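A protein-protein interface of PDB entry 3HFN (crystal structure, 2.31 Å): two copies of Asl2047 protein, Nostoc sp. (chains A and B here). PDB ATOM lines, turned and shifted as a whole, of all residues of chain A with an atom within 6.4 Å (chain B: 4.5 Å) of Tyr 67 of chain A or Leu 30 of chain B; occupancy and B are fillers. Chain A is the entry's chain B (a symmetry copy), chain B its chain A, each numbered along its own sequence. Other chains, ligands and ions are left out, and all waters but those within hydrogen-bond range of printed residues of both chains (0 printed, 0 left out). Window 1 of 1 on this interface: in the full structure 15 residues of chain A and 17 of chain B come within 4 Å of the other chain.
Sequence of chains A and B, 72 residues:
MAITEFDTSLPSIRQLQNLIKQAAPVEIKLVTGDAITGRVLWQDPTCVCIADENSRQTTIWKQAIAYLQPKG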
ATOM      1  N   GLU A  27      27.523  -5.621 -17.663  1.00  0.00           N
ATOM      2  CA  GLU A  27      27.322  -4.176 -17.841  1.00  0.00           C
ATOM      3  C   GLU A  27      25.894  -3.683 -17.423  1.00  0.00           C
ATOM      4  O   GLU A  27      24.852  -4.238 -17.788  1.00  0.00           O
ATOM      5  CB  GLU A  27      27.650  -3.760 -19.255  1.00  0.00           C
ATOM      6  CG  GLU A  27      27.428  -2.291 -19.532  1.00  0.00           C
ATOM      7  CD  GLU A  27      27.348  -2.010 -20.997  1.00  0.00           C
ATOM      8  OE1 GLU A  27      26.537  -2.645 -21.709  1.00  0.00           O
ATOM      9  OE2 GLU A  27      28.113  -1.134 -21.421  1.00  0.00           O
ATOM     10  N   ILE A  28      25.878  -2.629 -16.620  1.00  0.00           N
ATOM     11  CA  ILE A  28      24.639  -1.949 -16.265  1.00  0.00           C
ATOM     12  C   ILE A  28      24.610  -0.547 -16.893  1.00  0.00           C
ATOM     13  O   ILE A  28      25.485   0.275 -16.633  1.00  0.00           O
ATOM     14  CB  ILE A  28      24.499  -1.860 -14.750  1.00  0.00           C
ATOM     15  CG1 ILE A  28      24.903  -3.217 -14.148  1.00  0.00           C
ATOM     16  CG2 ILE A  28      23.086  -1.273 -14.379  1.00  0.00           C
ATOM     17  CD1 ILE A  28      24.629  -3.420 -12.704  1.00  0.00           C
ATOM     18  N   LYS A  29      23.610  -0.287 -17.739  1.00  0.00           N
ATOM     19  CA  LYS A  29      23.623   0.969 -18.465  1.00  0.00           C
ATOM     20  C   LYS A  29      22.745   1.867 -17.655  1.00  0.00           C
ATOM     21  O   LYS A  29      21.586   1.537 -17.366  1.00  0.00           O
ATOM     22  CB  LYS A  29      23.125   0.837 -19.900  1.00  0.00           C
ATOM     23  CG  LYS A  29      23.463   1.999 -20.784  1.00  0.00           C
ATOM     24  CD  LYS A  29      24.827   1.815 -21.457  1.00  0.00           C
ATOM     25  CE  LYS A  29      25.207   2.998 -22.328  1.00  0.00           C
ATOM     26  NZ  LYS A  29      24.128   3.277 -23.308  1.00  0.00           N
ATOM     27  N   LEU A  30      23.335   3.001 -17.264  1.00  0.00           N
ATOM     28  CA  LEU A  30      22.624   3.979 -16.446  1.00  0.00           C
ATOM     29  C   LEU A  30      21.904   4.901 -17.369  1.00  0.00           C
ATOM     30  O   LEU A  30      22.028   4.783 -18.584  1.00  0.00           O
ATOM     31  CB  LEU A  30      23.512   4.696 -15.426  1.00  0.00           C
ATOM     32  CG  LEU A  30      23.550   4.080 -13.988  1.00  0.00           C
ATOM     33  CD1 LEU A  30      23.269   2.573 -13.913  1.00  0.00           C
ATOM     34  CD2 LEU A  30      24.869   4.419 -13.311  1.00  0.00           C
ATOM     35  N   ALA A  64      18.283   4.648 -11.465  1.00  0.00           N
ATOM     36  CA  ALA A  64      19.002   5.147 -12.645  1.00  0.00           C
ATOM     37  C   ALA A  64      19.254   4.078 -13.750  1.00  0.00           C
ATOM     38  O   ALA A  64      19.737   4.458 -14.803  1.00  0.00           O
ATOM     39  CB  ALA A  64      20.288   5.753 -12.227  1.00  0.00           C
ATOM     40  N   ILE A  65      18.927   2.785 -13.510  1.00  0.00           N
ATOM     41  CA  ILE A  65      19.114   1.666 -14.426  1.00  0.00           C
ATOM     42  C   ILE A  65      18.159   1.671 -15.582  1.00  0.00           C
ATOM     43  O   ILE A  65      16.917   1.578 -15.412  1.00  0.00           O
ATOM     44  CB  ILE A  65      19.027   0.218 -13.751  1.00  0.00           C
ATOM     45  CG1 ILE A  65      20.022   0.121 -12.609  1.00  0.00           C
ATOM     46  CG2 ILE A  65      19.296  -0.984 -14.791  1.00  0.00           C
ATOM     47  CD1 ILE A  65      19.693  -0.902 -11.629  1.00  0.00           C
ATOM     48  N   ALA A  66      18.788   1.763 -16.757  1.00  0.00           N
ATOM     49  CA  ALA A  66      18.180   1.533 -18.094  1.00  0.00           C
ATOM     50  C   ALA A  66      18.062   0.014 -18.372  1.00  0.00           C
ATOM     51  O   ALA A  66      17.010  -0.509 -18.647  1.00  0.00           O
ATOM     52  CB  ALA A  66      19.031   2.197 -19.189  1.00  0.00           C
ATOM     53  N   TYR A  67      19.198  -0.660 -18.305  1.00  0.00           N
ATOM     54  CA  TYR A  67      19.292  -2.037 -18.626  1.00  0.00           C
ATOM     55  C   TYR A  67      20.569  -2.660 -18.216  1.00  0.00           C
ATOM     56  O   TYR A  67      21.618  -2.002 -18.114  1.00  0.00           O
ATOM     57  CB  TYR A  67      19.138  -2.268 -20.138  1.00  0.00           C
ATOM     58  CG  TYR A  67      20.299  -1.870 -21.038  1.00  0.00           C
ATOM     59  CD1 TYR A  67      21.534  -2.484 -20.943  1.00  0.00           C
ATOM     60  CD2 TYR A  67      20.127  -0.907 -22.027  1.00  0.00           C
ATOM     61  CE1 TYR A  67      22.575  -2.151 -21.798  1.00  0.00           C
ATOM     62  CE2 TYR A  67      21.176  -0.583 -22.889  1.00  0.00           C
ATOM     63  CZ  TYR A  67      22.375  -1.206 -22.763  1.00  0.00           C
ATOM     64  OH  TYR A  67      23.380  -0.823 -23.576  1.00  0.00           O
ATOM     65  N   LEU A  68      20.465  -3.987 -18.082  1.00  0.00           N
ATOM     66  CA  LEU A  68      21.525  -4.871 -17.651  1.00  0.00           C
ATOM     67  C   LEU A  68      21.775  -5.961 -18.692  1.00  0.00           C
ATOM     68  O   LEU A  68      20.873  -6.580 -19.194  1.00  0.00           O
ATOM     69  CB  LEU A  68      21.131  -5.524 -16.331  1.00  0.00           C
ATOM     70  CG  LEU A  68      22.038  -6.700 -15.964  1.00  0.00           C
ATOM     71  CD1 LEU A  68      22.142  -6.861 -14.483  1.00  0.00           C
ATOM     72  CD2 LEU A  68      21.519  -7.943 -16.530  1.00  0.00           C
ATOM     73  N   GLN A  69      23.033  -6.206 -19.005  1.00  0.00           N
ATOM     74  CA  GLN A  69      23.401  -7.361 -19.806  1.00  0.00           C
ATOM     75  C   GLN A  69      24.561  -8.198 -19.243  1.00  0.00           C
ATOM     76  O   GLN A  69      25.644  -7.687 -18.975  1.00  0.00           O
ATOM     77  CB  GLN A  69      23.833  -6.926 -21.183  1.00  0.00           C
ATOM     78  CG  GLN A  69      23.252  -5.669 -21.773  1.00  0.00           C
ATOM     79  CD  GLN A  69      23.534  -5.615 -23.265  1.00  0.00           C
ATOM     80  OE1 GLN A  69      24.511  -6.147 -23.725  1.00  0.00           O
ATOM     81  NE2 GLN A  69      22.672  -4.976 -24.012  1.00  0.00           N
ATOM     82  N   ILE B  28      12.258  -1.730 -28.466  1.00  0.00           N
ATOM     83  CA  ILE B  28      11.914  -1.044 -27.205  1.00  0.00           C
ATOM     84  C   ILE B  28      12.725   0.244 -27.107  1.00  0.00           C
ATOM     85  O   ILE B  28      13.955   0.204 -26.972  1.00  0.00           O
ATOM     86  CB  ILE B  28      12.289  -1.927 -26.002  1.00  0.00           C
ATOM     87  CG1 ILE B  28      11.630  -3.326 -26.107  1.00  0.00           C
ATOM     88  CG2 ILE B  28      11.951  -1.195 -24.696  1.00  0.00           C
ATOM     89  CD1 ILE B  28      12.478  -4.417 -25.590  1.00  0.00           C
ATOM     90  N   LYS B  29      12.048   1.386 -27.149  1.00  0.00           N
ATOM     91  CA  LYS B  29      12.786   2.644 -27.148  1.00  0.00           C
ATOM     92  C   LYS B  29      12.887   3.129 -25.739  1.00  0.00           C
ATOM     93  O   LYS B  29      11.908   3.546 -25.137  1.00  0.00           O
ATOM     94  CB  LYS B  29      12.162   3.725 -28.027  1.00  0.00           C
ATOM     95  CG  LYS B  29      13.064   4.897 -28.343  1.00  0.00           C
ATOM     96  CD  LYS B  29      13.826   4.638 -29.642  1.00  0.00           C
ATOM     97  CE  LYS B  29      14.879   5.732 -30.002  1.00  0.00           C
ATOM     98  NZ  LYS B  29      14.411   7.135 -29.873  1.00  0.00           N
ATOM     99  N   LEU B  30      14.103   3.052 -25.227  1.00  0.00           N
ATOM    100  CA  LEU B  30      14.410   3.495 -23.881  1.00  0.00           C
ATOM    101  C   LEU B  30      14.541   4.996 -23.883  1.00  0.00           C
ATOM    102  O   LEU B  30      14.810   5.596 -24.907  1.00  0.00           O
ATOM    103  CB  LEU B  30      15.649   2.787 -23.338  1.00  0.00           C
ATOM    104  CG  LEU B  30      15.508   1.453 -22.538  1.00  0.00           C
ATOM    105  CD1 LEU B  30      14.292   0.621 -22.878  1.00  0.00           C
ATOM    106  CD2 LEU B  30      16.769   0.655 -22.694  1.00  0.00           C
ATOM    107  N   VAL B  31      14.301   5.605 -22.739  1.00  0.00           N
ATOM    108  CA  VAL B  31      14.218   7.057 -22.603  1.00  0.00           C
ATOM    109  C   VAL B  31      15.560   7.691 -22.770  1.00  0.00           C
ATOM    110  O   VAL B  31      15.701   8.925 -22.609  1.00  0.00           O
ATOM    111  CB  VAL B  31      13.616   7.456 -21.237  1.00  0.00           C
ATOM    112  CG1 VAL B  31      12.349   6.665 -20.998  1.00  0.00           C
ATOM    113  CG2 VAL B  31      14.591   7.195 -20.106  1.00  0.00           C
ATOM    114  N   THR B  32      16.524   6.821 -23.102  1.00  0.00           N
ATOM    115  CA  THR B  32      17.953   7.134 -23.356  1.00  0.00           C
ATOM    116  C   THR B  32      18.217   7.412 -24.829  1.00  0.00           C
ATOM    117  O   THR B  32      19.179   8.079 -25.157  1.00  0.00           O
ATOM    118  CB  THR B  32      18.865   5.945 -22.909  1.00  0.00           C
ATOM    119  OG1 THR B  32      18.602   5.630 -21.545  1.00  0.00           O
ATOM    120  CG2 THR B  32      20.299   6.274 -23.017  1.00  0.00           C
ATOM    121  N   GLY B  33      17.357   6.895 -25.713  1.00  0.00           N
ATOM    122  CA  GLY B  33      17.660   6.815 -27.142  1.00  0.00           C
ATOM    123  C   GLY B  33      18.094   5.417 -27.507  1.00  0.00           C
ATOM    124  O   GLY B  33      18.628   5.193 -28.575  1.00  0.00           O
ATOM    125  N   ASP B  34      17.893   4.479 -26.601  1.00  0.00           N
ATOM    126  CA  ASP B  34      18.358   3.127 -26.784  1.00  0.00           C
ATOM    127  C   ASP B  34      17.295   2.311 -27.513  1.00  0.00           C
ATOM    128  O   ASP B  34      16.446   1.664 -26.845  1.00  0.00           O
ATOM    129  CB  ASP B  34      18.627   2.429 -25.416  1.00  0.00           C
ATOM    130  CG  ASP B  34      19.991   2.840 -24.743  1.00  0.00           C
ATOM    131  OD1 ASP B  34      21.088   2.673 -25.340  1.00  0.00           O
ATOM    132  OD2 ASP B  34      19.965   3.271 -23.550  1.00  0.00           O
ATOM    133  N   ILE B  36      16.217  -0.888 -28.685  1.00  0.00           N
ATOM    134  CA  ILE B  36      16.715  -2.209 -28.351  1.00  0.00           C
ATOM    135  C   ILE B  36      16.062  -3.219 -29.248  1.00  0.00           C
ATOM    136  O   ILE B  36      14.898  -3.476 -29.153  1.00  0.00           O
ATOM    137  CB  ILE B  36      16.539  -2.591 -26.817  1.00  0.00           C
ATOM    138  CG1 ILE B  36      17.237  -1.565 -25.876  1.00  0.00           C
ATOM    139  CG2 ILE B  36      16.970  -4.034 -26.578  1.00  0.00           C
ATOM    140  CD1 ILE B  36      18.266  -2.163 -24.870  1.00  0.00           C
ATOM    141  N   THR B  58      19.873  -8.536 -22.527  1.00  0.00           N
ATOM    142  CA  THR B  58      19.818  -7.189 -22.002  1.00  0.00           C
ATOM    143  C   THR B  58      18.581  -7.016 -21.248  1.00  0.00           C
ATOM    144  O   THR B  58      17.645  -6.497 -21.811  1.00  0.00           O
ATOM    145  CB  THR B  58      19.819  -6.105 -23.148  1.00  0.00           C
ATOM    146  OG1 THR B  58      19.228  -4.874 -22.722  1.00  0.00           O
ATOM    147  CG2 THR B  58      19.093  -6.600 -24.376  1.00  0.00           C
ATOM    148  N   THR B  59      18.548  -7.365 -19.969  1.00  0.00           N
ATOM    149  CA  THR B  59      17.382  -6.996 -19.146  1.00  0.00           C
ATOM    150  C   THR B  59      17.226  -5.482 -18.987  1.00  0.00           C
ATOM    151  O   THR B  59      18.221  -4.796 -18.771  1.00  0.00           O
ATOM    152  CB  THR B  59      17.276  -7.845 -17.899  1.00  0.00           C
ATOM    153  OG1 THR B  59      17.765  -7.169 -16.745  1.00  0.00           O
ATOM    154  CG2 THR B  59      18.060  -9.086 -18.148  1.00  0.00           C
ATOM    155  N   ILE B  60      15.980  -4.991 -19.219  1.00  0.00           N
ATOM    156  CA  ILE B  60      15.600  -3.547 -19.262  1.00  0.00           C
ATOM    157  C   ILE B  60      14.769  -3.229 -18.045  1.00  0.00           C
ATOM    158  O   ILE B  60      14.083  -4.149 -17.562  1.00  0.00           O
ATOM    159  CB  ILE B  60      14.785  -3.182 -20.518  1.00  0.00           C
ATOM    160  CG1 ILE B  60      15.528  -3.631 -21.757  1.00  0.00           C
ATOM    161  CG2 ILE B  60      14.561  -1.693 -20.620  1.00  0.00           C
ATOM    162  CD1 ILE B  60      14.905  -3.302 -23.062  1.00  0.00           C
ATOM    163  N   ALA B  64      12.867   2.736 -17.668  1.00  0.00           N
ATOM    164  CA  ALA B  64      13.562   3.456 -18.733  1.00  0.00           C
ATOM    165  C   ALA B  64      12.807   3.299 -20.067  1.00  0.00           C
ATOM    166  O   ALA B  64      13.384   3.562 -21.095  1.00  0.00           O
ATOM    167  CB  ALA B  64      14.876   2.919 -18.897  1.00  0.00           C
ATOM    168  N   ILE B  65      11.550   2.872 -20.028  1.00  0.00           N
ATOM    169  CA  ILE B  65      10.764   2.577 -21.149  1.00  0.00           C
ATOM    170  C   ILE B  65       9.876   3.697 -21.692  1.00  0.00           C
ATOM    171  O   ILE B  65       8.977   4.199 -21.028  1.00  0.00           O
ATOM    172  CB  ILE B  65       9.957   1.286 -21.073  1.00  0.00           C
ATOM    173  CG1 ILE B  65      10.944   0.060 -21.048  1.00  0.00           C
ATOM    174  CG2 ILE B  65       9.285   1.175 -22.353  1.00  0.00           C
ATOM    175  CD1 ILE B  65      10.218  -1.357 -20.894  1.00  0.00           C
ATOM    176  N   ALA B  66      10.098   4.100 -22.937  1.00  0.00           N
ATOM    177  CA  ALA B  66       9.342   5.185 -23.498  1.00  0.00           C
ATOM    178  C   ALA B  66       8.219   4.545 -24.252  1.00  0.00           C
ATOM    179  O   ALA B  66       7.050   4.919 -24.120  1.00  0.00           O
ATOM    180  CB  ALA B  66      10.241   5.967 -24.467  1.00  0.00           C
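Printed residues of chain A that touch a printed residue of chain B: Lys 29, Ala 66, Tyr 67, Leu 68 and Gln 69. Hydrophobic or aromatic side chains of chain A that line the printed part of chain B: Tyr 67 and Leu 68. Of the 14 printed residues of chain B, 7 touch a printed residue of chain A. Among the printed residues, 11 pairs touch across the chains.
O of Lys 29 of chain A sits at hydrogen-bond distance from N of Ala 66 of chain A. The side-chain carboxylate of Asp 34 of chain B lies close to the side-chain hydroxyl of Thr 32 of chain B (3.4 Å). The backbone carbonyl oxygen (O) of Ala 64 of chain B sits at hydrogen-bond distance from the backbone NH (N) of Val 31 of chain B, 2.8 Å away. The backbone carbonyl oxygen (O) of Tyr 67 of chain A is in hydrogen-bond range of the backbone NH (N) of Lys 29 of chain A (2.7 Å). N of Gln 69 of chain A is in hydrogen-bond range of O of Glu 27 of chain A (2.9 Å). N of Ile 36 of chain B is in hydrogen-bond range of O of Ile 28 of chain B (3.0 Å).
Ala 66 of chain A touches Ala 64 of chain B, but with the chains exchanged Ala 64 of chain A does not touch Ala 66 of chain B (12.6 Å). 6 positions are printed for both chains.
Leu 30 of chain B touches just one residue of chain A: Tyr 67. Of the printed residues of chain A, Thr 58 of chain B touches Tyr 67, Leu 68 and Gln 69. Printed residues of chain B within 4 Å of Leu 68 of chain A: Thr 58 and Thr 59. Of the printed residues of chain A, Ile 60 of chain B touches Ala 66 and Tyr 67. Printed residues of chain A within 4 Å of Ile 36 of chain B: Tyr 67. Ile 28 of chain A touches none of the printed residues of chain B. Ile 65 of chain B touches none of the printed residues of chain A. The nearest residue of chain A that does not touch Leu 30 of chain B is Ala 66 of chain A (4.2 Å). The nearest printed residue of chain A that does not touch Ile 60 of chain B is Leu 68 of chain A (4.7 Å).
O of Thr 59 of chain B lies within hydrogen-bond range of N of Leu 68 of chain A, 2.5 Å away. The side-chain carboxylate (OD1) of Asp 34 of chain B lies within salt-bridge range of the side-chain amino group (NZ) of Lys 29 of chain A, at 3.7 Å.
Among the printed residues, pairs that only touch across the chains: Tyr 67 of chain A with Thr 59 of chain B (3.0 Å), Leu 68 of chain A with Thr 58 of chain B (3.1 Å), Gln 69 of chain A with Thr 58 of chain B (3.2 Å), Ala 66 of chain A with Ile 60 of chain B (3.4 Å), Tyr 67 of chain A with Thr 58 of chain B (3.6 Å), Tyr 67 of chain A with Ile 36 of chain B (3.6 Å), Ala 66 of chain A with Ala 64 of chain B (3.7 Å), Tyr 67 of chain A with Leu 30 of chain B (3.8 Å) and Tyr 67 of chain A with Ile 60 of chain B (3.9 Å).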
